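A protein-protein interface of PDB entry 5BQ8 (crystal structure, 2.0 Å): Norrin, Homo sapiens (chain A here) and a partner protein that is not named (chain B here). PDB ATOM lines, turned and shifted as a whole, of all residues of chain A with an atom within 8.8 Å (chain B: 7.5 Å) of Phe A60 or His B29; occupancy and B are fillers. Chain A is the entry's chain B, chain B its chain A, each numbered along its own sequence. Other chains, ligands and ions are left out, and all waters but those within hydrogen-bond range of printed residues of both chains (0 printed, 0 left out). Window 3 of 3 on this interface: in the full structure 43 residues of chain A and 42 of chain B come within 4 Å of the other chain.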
ATOM      1  N   LEU A  57      30.351   1.933  11.359  1.00  0.00           N
ATOM      2  CA  LEU A  57      30.072   0.517  11.542  1.00  0.00           C
ATOM      3  C   LEU A  57      30.038   0.249  13.030  1.00  0.00           C
ATOM      4  O   LEU A  57      30.818   0.838  13.778  1.00  0.00           O
ATOM      5  CB  LEU A  57      31.140  -0.351  10.874  1.00  0.00           C
ATOM      6  CG  LEU A  57      31.079  -0.485   9.353  1.00  0.00           C
ATOM      7  CD1 LEU A  57      32.359  -1.118   8.826  1.00  0.00           C
ATOM      8  CD2 LEU A  57      29.868  -1.308   8.937  1.00  0.00           C
ATOM      9  N   VAL A  58      29.138  -0.626  13.464  1.00  0.00           N
ATOM     10  CA  VAL A  58      29.027  -0.938  14.881  1.00  0.00           C
ATOM     11  C   VAL A  58      29.922  -2.120  15.226  1.00  0.00           C
ATOM     12  O   VAL A  58      29.838  -3.185  14.618  1.00  0.00           O
ATOM     13  CB  VAL A  58      27.578  -1.267  15.280  1.00  0.00           C
ATOM     14  CG1 VAL A  58      27.491  -1.564  16.778  1.00  0.00           C
ATOM     15  CG2 VAL A  58      26.656  -0.116  14.908  1.00  0.00           C
ATOM     16  N   SER A  59      30.764  -1.926  16.230  1.00  0.00           N
ATOM     17  CA  SER A  59      31.631  -2.986  16.707  1.00  0.00           C
ATOM     18  C   SER A  59      31.079  -3.534  18.012  1.00  0.00           C
ATOM     19  O   SER A  59      30.394  -2.829  18.753  1.00  0.00           O
ATOM     20  CB  SER A  59      33.062  -2.477  16.892  1.00  0.00           C
ATOM     21  OG  SER A  59      33.728  -2.423  15.646  1.00  0.00           O
ATOM     22  N   PHE A  60      31.389  -4.795  18.276  1.00  0.00           N
ATOM     23  CA  PHE A  60      31.004  -5.458  19.511  1.00  0.00           C
ATOM     24  C   PHE A  60      32.271  -6.048  20.123  1.00  0.00           C
ATOM     25  O   PHE A  60      33.339  -5.994  19.511  1.00  0.00           O
ATOM     26  CB  PHE A  60      29.941  -6.532  19.256  1.00  0.00           C
ATOM     27  CG  PHE A  60      28.690  -6.006  18.596  1.00  0.00           C
ATOM     28  CD1 PHE A  60      27.656  -5.485  19.357  1.00  0.00           C
ATOM     29  CD2 PHE A  60      28.547  -6.039  17.219  1.00  0.00           C
ATOM     30  CE1 PHE A  60      26.505  -5.004  18.756  1.00  0.00           C
ATOM     31  CE2 PHE A  60      27.398  -5.559  16.613  1.00  0.00           C
ATOM     32  CZ  PHE A  60      26.376  -5.042  17.384  1.00  0.00           C
ATOM     33  N   SER A  61      32.150  -6.611  21.321  1.00  0.00           N
ATOM     34  CA  SER A  61      33.308  -7.084  22.076  1.00  0.00           C
ATOM     35  C   SER A  61      34.211  -8.033  21.289  1.00  0.00           C
ATOM     36  O   SER A  61      35.431  -7.897  21.326  1.00  0.00           O
ATOM     37  CB  SER A  61      32.838  -7.774  23.358  1.00  0.00           C
ATOM     38  OG  SER A  61      31.959  -6.931  24.085  1.00  0.00           O
ATOM     39  N   THR A  62      33.612  -8.974  20.569  1.00  0.00           N
ATOM     40  CA  THR A  62      34.364  -9.960  19.794  1.00  0.00           C
ATOM     41  C   THR A  62      34.229  -9.743  18.286  1.00  0.00           C
ATOM     42  O   THR A  62      34.715 -10.552  17.494  1.00  0.00           O
ATOM     43  CB  THR A  62      33.911 -11.389  20.128  1.00  0.00           C
ATOM     44  OG1 THR A  62      32.632 -11.634  19.532  1.00  0.00           O
ATOM     45  CG2 THR A  62      33.804 -11.583  21.632  1.00  0.00           C
ATOM     46  N   VAL A  63      33.572  -8.652  17.899  1.00  0.00           N
ATOM     47  CA  VAL A  63      33.370  -8.324  16.490  1.00  0.00           C
ATOM     48  C   VAL A  63      33.972  -6.955  16.192  1.00  0.00           C
ATOM     49  O   VAL A  63      33.290  -5.933  16.264  1.00  0.00           O
ATOM     50  CB  VAL A  63      31.877  -8.321  16.122  1.00  0.00           C
ATOM     51  CG1 VAL A  63      31.698  -8.186  14.617  1.00  0.00           C
ATOM     52  CG2 VAL A  63      31.210  -9.594  16.621  1.00  0.00           C
ATOM     53  N   LEU A  64      35.260  -6.957  15.859  1.00  0.00           N
ATOM     54  CA  LEU A  64      36.016  -5.734  15.610  1.00  0.00           C
ATOM     55  C   LEU A  64      36.028  -5.349  14.135  1.00  0.00           C
ATOM     56  O   LEU A  64      36.605  -6.047  13.302  1.00  0.00           O
ATOM     57  CB  LEU A  64      37.451  -5.904  16.112  1.00  0.00           C
ATOM     58  CG  LEU A  64      37.688  -5.478  17.563  1.00  0.00           C
ATOM     59  CD1 LEU A  64      36.668  -6.121  18.485  1.00  0.00           C
ATOM     60  CD2 LEU A  64      39.101  -5.828  18.005  1.00  0.00           C
ATOM     61  N   MLY A  65      35.397  -4.221  13.828  1.00  0.00           N
ATOM     62  CA  MLY A  65      35.264  -3.750  12.459  1.00  0.00           C
ATOM     63  CB  MLY A  65      33.783  -3.548  12.127  1.00  0.00           C
ATOM     64  CG  MLY A  65      32.993  -4.844  11.983  1.00  0.00           C
ATOM     65  CD  MLY A  65      31.548  -4.695  12.463  1.00  0.00           C
ATOM     66  CE  MLY A  65      30.548  -5.094  11.385  1.00  0.00           C
ATOM     67  NZ  MLY A  65      29.166  -5.318  11.922  1.00  0.00           N
ATOM     68  CH1 MLY A  65      28.453  -4.031  11.938  1.00  0.00           C
ATOM     69  CH2 MLY A  65      28.454  -6.142  10.938  1.00  0.00           C
ATOM     70  C   MLY A  65      36.006  -2.435  12.278  1.00  0.00           C
ATOM     71  O   MLY A  65      36.298  -1.742  13.252  1.00  0.00           O
ATOM     72  N   SER B  26      18.730   1.146  14.830  1.00  0.00           N
ATOM     73  CA  SER B  26      18.624   0.288  15.993  1.00  0.00           C
ATOM     74  C   SER B  26      19.867  -0.579  16.022  1.00  0.00           C
ATOM     75  O   SER B  26      20.162  -1.269  15.048  1.00  0.00           O
ATOM     76  CB  SER B  26      17.365  -0.576  15.951  1.00  0.00           C
ATOM     77  OG  SER B  26      17.417  -1.488  14.869  1.00  0.00           O
ATOM     78  N   ILE B  27      20.591  -0.559  17.135  1.00  0.00           N
ATOM     79  CA  ILE B  27      21.813  -1.338  17.229  1.00  0.00           C
ATOM     80  C   ILE B  27      21.438  -2.685  17.810  1.00  0.00           C
ATOM     81  O   ILE B  27      20.887  -2.777  18.907  1.00  0.00           O
ATOM     82  CB  ILE B  27      22.870  -0.636  18.105  1.00  0.00           C
ATOM     83  CG1 ILE B  27      23.403   0.604  17.382  1.00  0.00           C
ATOM     84  CG2 ILE B  27      24.025  -1.578  18.429  1.00  0.00           C
ATOM     85  CD1 ILE B  27      24.253   1.512  18.243  1.00  0.00           C
ATOM     86  N   SER B  28      21.756  -3.728  17.055  1.00  0.00           N
ATOM     87  CA  SER B  28      21.483  -5.093  17.461  1.00  0.00           C
ATOM     88  C   SER B  28      22.672  -5.981  17.134  1.00  0.00           C
ATOM     89  O   SER B  28      23.389  -5.747  16.164  1.00  0.00           O
ATOM     90  CB  SER B  28      20.221  -5.609  16.767  1.00  0.00           C
ATOM     91  OG  SER B  28      20.444  -5.803  15.383  1.00  0.00           O
ATOM     92  N   HIS B  29      22.889  -6.990  17.963  1.00  0.00           N
ATOM     93  CA  HIS B  29      23.975  -7.928  17.742  1.00  0.00           C
ATOM     94  C   HIS B  29      23.642  -8.865  16.578  1.00  0.00           C
ATOM     95  O   HIS B  29      22.527  -9.378  16.495  1.00  0.00           O
ATOM     96  CB  HIS B  29      24.259  -8.710  19.021  1.00  0.00           C
ATOM     97  CG  HIS B  29      25.595  -9.379  19.030  1.00  0.00           C
ATOM     98  ND1 HIS B  29      25.866 -10.508  18.290  1.00  0.00           N
ATOM     99  CD2 HIS B  29      26.751  -9.052  19.654  1.00  0.00           C
ATOM    100  CE1 HIS B  29      27.121 -10.868  18.481  1.00  0.00           C
ATOM    101  NE2 HIS B  29      27.684  -9.998  19.300  1.00  0.00           N
ATOM    102  N   PRO B  30      24.604  -9.085  15.665  1.00  0.00           N
ATOM    103  CA  PRO B  30      24.301  -9.880  14.468  1.00  0.00           C
ATOM    104  C   PRO B  30      24.040 -11.364  14.731  1.00  0.00           C
ATOM    105  O   PRO B  30      23.486 -12.029  13.854  1.00  0.00           O
ATOM    106  CB  PRO B  30      25.566  -9.708  13.613  1.00  0.00           C
ATOM    107  CG  PRO B  30      26.642  -9.388  14.588  1.00  0.00           C
ATOM    108  CD  PRO B  30      25.973  -8.541  15.628  1.00  0.00           C
ATOM    109  N   LEU B  31      24.454 -11.880  15.885  1.00  0.00           N
ATOM    110  CA  LEU B  31      24.260 -13.295  16.204  1.00  0.00           C
ATOM    111  C   LEU B  31      23.354 -13.539  17.409  1.00  0.00           C
ATOM    112  O   LEU B  31      22.482 -14.408  17.375  1.00  0.00           O
ATOM    113  CB  LEU B  31      25.606 -13.972  16.460  1.00  0.00           C
ATOM    114  CG  LEU B  31      25.511 -15.485  16.686  1.00  0.00           C
ATOM    115  CD1 LEU B  31      25.006 -16.188  15.431  1.00  0.00           C
ATOM    116  CD2 LEU B  31      26.847 -16.062  17.132  1.00  0.00           C
ATOM    117  N   TYR B  32      23.568 -12.769  18.472  1.00  0.00           N
ATOM    118  CA  TYR B  32      22.830 -12.945  19.719  1.00  0.00           C
ATOM    119  C   TYR B  32      21.566 -12.096  19.723  1.00  0.00           C
ATOM    120  O   TYR B  32      21.624 -10.887  19.513  1.00  0.00           O
ATOM    121  CB  TYR B  32      23.710 -12.572  20.913  1.00  0.00           C
ATOM    122  CG  TYR B  32      24.989 -13.375  21.014  1.00  0.00           C
ATOM    123  CD1 TYR B  32      24.978 -14.760  20.924  1.00  0.00           C
ATOM    124  CD2 TYR B  32      26.211 -12.740  21.187  1.00  0.00           C
ATOM    125  CE1 TYR B  32      26.151 -15.491  21.013  1.00  0.00           C
ATOM    126  CE2 TYR B  32      27.387 -13.459  21.273  1.00  0.00           C
ATOM    127  CZ  TYR B  32      27.352 -14.833  21.186  1.00  0.00           C
ATOM    128  OH  TYR B  32      28.524 -15.551  21.275  1.00  0.00           O
ATOM    129  N   LYS B  33      20.424 -12.735  19.954  1.00  0.00           N
ATOM    130  CA  LYS B  33      19.149 -12.028  20.001  1.00  0.00           C
ATOM    131  C   LYS B  33      19.066 -11.175  21.264  1.00  0.00           C
ATOM    132  O   LYS B  33      18.593 -11.635  22.305  1.00  0.00           O
ATOM    133  CB  LYS B  33      17.991 -13.026  19.938  1.00  0.00           C
ATOM    134  CG  LYS B  33      16.614 -12.392  19.914  1.00  0.00           C
ATOM    135  CD  LYS B  33      15.581 -13.388  19.409  1.00  0.00           C
ATOM    136  CE  LYS B  33      14.163 -12.859  19.531  1.00  0.00           C
ATOM    137  NZ  LYS B  33      13.165 -13.940  19.303  1.00  0.00           N
ATOM    138  N   CYS B  34      19.532  -9.932  21.166  1.00  0.00           N
ATOM    139  CA  CYS B  34      19.621  -9.049  22.325  1.00  0.00           C
ATOM    140  C   CYS B  34      18.532  -7.978  22.343  1.00  0.00           C
ATOM    141  O   CYS B  34      17.654  -7.947  21.481  1.00  0.00           O
ATOM    142  CB  CYS B  34      20.995  -8.383  22.350  1.00  0.00           C
ATOM    143  SG  CYS B  34      22.359  -9.561  22.386  1.00  0.00           S
ATOM    144  N   SER B  35      18.616  -7.097  23.335  1.00  0.00           N
ATOM    145  CA  SER B  35      17.710  -5.964  23.481  1.00  0.00           C
ATOM    146  C   SER B  35      18.144  -4.812  22.597  1.00  0.00           C
ATOM    147  O   SER B  35      18.923  -3.964  23.030  1.00  0.00           O
ATOM    148  CB  SER B  35      17.666  -5.492  24.932  1.00  0.00           C
ATOM    149  OG  SER B  35      18.951  -5.062  25.349  1.00  0.00           O
ATOM    150  N   SER B  36      17.655  -4.782  21.363  1.00  0.00           N
ATOM    151  CA  SER B  36      18.053  -3.742  20.426  1.00  0.00           C
ATOM    152  C   SER B  36      17.781  -2.361  21.013  1.00  0.00           C
ATOM    153  O   SER B  36      16.891  -2.191  21.848  1.00  0.00           O
ATOM    154  CB  SER B  36      17.314  -3.907  19.100  1.00  0.00           C
ATOM    155  OG  SER B  36      17.635  -5.149  18.498  1.00  0.00           O
ATOM    156  N   LEU B  85      27.706   1.547  24.292  1.00  0.00           N
ATOM    157  CA  LEU B  85      26.439   1.346  24.979  1.00  0.00           C
ATOM    158  C   LEU B  85      26.276  -0.136  25.250  1.00  0.00           C
ATOM    159  O   LEU B  85      26.771  -0.973  24.491  1.00  0.00           O
ATOM    160  CB  LEU B  85      25.266   1.905  24.169  1.00  0.00           C
ATOM    161  CG  LEU B  85      24.929   1.343  22.790  1.00  0.00           C
ATOM    162  CD1 LEU B  85      24.117   0.056  22.873  1.00  0.00           C
ATOM    163  CD2 LEU B  85      24.169   2.389  22.003  1.00  0.00           C
ATOM    164  N   LEU B  87      24.096  -3.531  25.631  1.00  0.00           N
ATOM    165  CA  LEU B  87      22.858  -4.234  25.303  1.00  0.00           C
ATOM    166  C   LEU B  87      22.559  -5.309  26.349  1.00  0.00           C
ATOM    167  O   LEU B  87      23.449  -5.747  27.081  1.00  0.00           O
ATOM    168  CB  LEU B  87      22.909  -4.871  23.912  1.00  0.00           C
ATOM    169  CG  LEU B  87      23.134  -3.940  22.719  1.00  0.00           C
ATOM    170  CD1 LEU B  87      23.106  -4.746  21.429  1.00  0.00           C
ATOM    171  CD2 LEU B  87      22.130  -2.800  22.684  1.00  0.00           C
ATOM    172  N   CYS B  89      20.956  -9.152  26.718  1.00  0.00           N
ATOM    173  CA  CYS B  89      20.676 -10.324  25.901  1.00  0.00           C
ATOM    174  C   CYS B  89      20.267 -11.508  26.768  1.00  0.00           C
ATOM    175  O   CYS B  89      20.273 -11.425  27.996  1.00  0.00           O
ATOM    176  CB  CYS B  89      21.915 -10.701  25.089  1.00  0.00           C
ATOM    177  SG  CYS B  89      22.773  -9.296  24.353  1.00  0.00           S
ATOM    178  N   LEU B  95      26.512  -7.148  26.598  1.00  0.00           N
ATOM    179  CA  LEU B  95      27.426  -6.910  25.489  1.00  0.00           C
ATOM    180  C   LEU B  95      27.588  -5.431  25.200  1.00  0.00           C
ATOM    181  O   LEU B  95      26.606  -4.693  25.099  1.00  0.00           O
ATOM    182  CB  LEU B  95      26.933  -7.621  24.227  1.00  0.00           C
ATOM    183  CG  LEU B  95      26.706  -9.127  24.326  1.00  0.00           C
ATOM    184  CD1 LEU B  95      26.235  -9.660  22.990  1.00  0.00           C
ATOM    185  CD2 LEU B  95      27.983  -9.838  24.753  1.00  0.00           C
ATOM    186  N   THR B  96      28.837  -5.006  25.075  1.00  0.00           N
ATOM    187  CA  THR B  96      29.132  -3.626  24.745  1.00  0.00           C
ATOM    188  C   THR B  96      29.129  -3.507  23.229  1.00  0.00           C
ATOM    189  O   THR B  96      29.658  -4.372  22.528  1.00  0.00           O
ATOM    190  CB  THR B  96      30.482  -3.166  25.316  1.00  0.00           C
ATOM    191  OG1 THR B  96      30.471  -3.307  26.740  1.00  0.00           O
ATOM    192  CG2 THR B  96      30.743  -1.710  24.964  1.00  0.00           C
ATOM    193  N   ALA B  97      28.551  -2.422  22.732  1.00  0.00           N
ATOM    194  CA  ALA B  97      28.580  -2.106  21.316  1.00  0.00           C
ATOM    195  C   ALA B  97      29.250  -0.757  21.197  1.00  0.00           C
ATOM    196  O   ALA B  97      29.082   0.090  22.066  1.00  0.00           O
ATOM    197  CB  ALA B  97      27.178  -2.082  20.723  1.00  0.00           C
ATOM    198  N   THR B  98      30.027  -0.571  20.138  1.00  0.00           N
ATOM    199  CA  THR B  98      30.789   0.654  19.962  1.00  0.00           C
ATOM    200  C   THR B  98      30.727   1.143  18.525  1.00  0.00           C
ATOM    201  O   THR B  98      30.588   0.355  17.593  1.00  0.00           O
ATOM    202  CB  THR B  98      32.260   0.452  20.348  1.00  0.00           C
ATOM    203  OG1 THR B  98      32.829  -0.559  19.511  1.00  0.00           O
ATOM    204  CG2 THR B  98      32.385   0.020  21.789  1.00  0.00           C
ATOM    205  N   TYR B  99      30.846   2.453  18.355  1.00  0.00           N
ATOM    206  CA  TYR B  99      30.722   3.074  17.049  1.00  0.00           C
ATOM    207  C   TYR B  99      31.206   4.511  17.137  1.00  0.00           C
ATOM    208  O   TYR B  99      31.285   5.081  18.222  1.00  0.00           O
ATOM    209  CB  TYR B  99      29.270   3.037  16.562  1.00  0.00           C
ATOM    210  CG  TYR B  99      28.325   3.809  17.458  1.00  0.00           C
ATOM    211  CD1 TYR B  99      28.130   5.174  17.283  1.00  0.00           C
ATOM    212  CD2 TYR B  99      27.643   3.177  18.489  1.00  0.00           C
ATOM    213  CE1 TYR B  99      27.275   5.887  18.103  1.00  0.00           C
ATOM    214  CE2 TYR B  99      26.786   3.882  19.317  1.00  0.00           C
ATOM    215  CZ  TYR B  99      26.605   5.236  19.117  1.00  0.00           C
ATOM    216  OH  TYR B  99      25.757   5.943  19.939  1.00  0.00           O
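The backbone NH (N) of Ser A59 lies within hydrogen-bond range of the backbone carbonyl oxygen (O) of Thr B98.
A ring nitrogen (ND1) of His B29 lies within hydrogen-bond range of the backbone NH (N) of Leu B31. A ring nitrogen (ND1) of His B29 sits at hydrogen-bond distance from the backbone NH (N) of Tyr B32 (3.2 Å). O of Leu B85 is in hydrogen-bond range of N of Ala B97 (2.9 Å). The side-chain hydroxyl of Ser A59 is in hydrogen-bond range of N of MLY A65, 3.1 Å away. The side-chain sulfur of Cys B34 forms a disulfide with the side-chain sulfur of Cys B89.
Among the printed residues, merely in contact across the chains: Ser A59 with Ala B97 (3.2 Å), Phe A60 with Ser B28 (3.3 Å), Val A58 with Thr B98 (3.4 Å), Phe A60 with Pro B30 (3.4 Å), Phe A60 with Thr B96 (3.5 Å), Ser A61 with Thr B96 (3.6 Å), Phe A60 with Ala B97 (3.6 Å), Phe A60 with His B29 (3.7 Å), Val A58 with Ile B27 (3.8 Å), Leu A57 with Thr B98 (3.9 Å), Leu A57 with Tyr B99 (3.9 Å) and Val A58 with Ala B97 (3.99 Å).
Of the printed residues of chain B, Leu A57 touches Thr B98 (3.9 Å) and Tyr B99 (3.9 Å). Ser B26 touches none of the printed residues of chain A. Printed residues of chain A within 4 Å of Ile B27: Val A58 (3.8 Å). His B29 touches one residue of chain A. Pro B30 touches just one residue of chain A: Phe A60 (3.4 Å). Ser B36 touches none of the printed residues of chain A. Printed residues of chain A within 4 Å of Tyr B99: Leu A57 (3.9 Å). The nearest printed residue of chain A that does not touch Tyr B99 is Val A58 (4.3 Å).
Of the 9 printed residues of chain A, 5 touch a printed residue of chain B. Printed residues of chain A that touch a printed residue of chain B: Leu A57, Val A58, Ser A59, Phe A60 and Ser A61. Printed residues of chain B that touch a printed residue of chain A: Ile B27, Ser B28, His B29, Pro B30, Thr B96, Ala B97, Thr B98 and Tyr B99. Among the printed residues, 13 pairs touch across the chains. Among the printed residues, no Asp or Glu carboxylate lies within 4 Å of a Lys or Arg side-chain nitrogen of the other chain.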
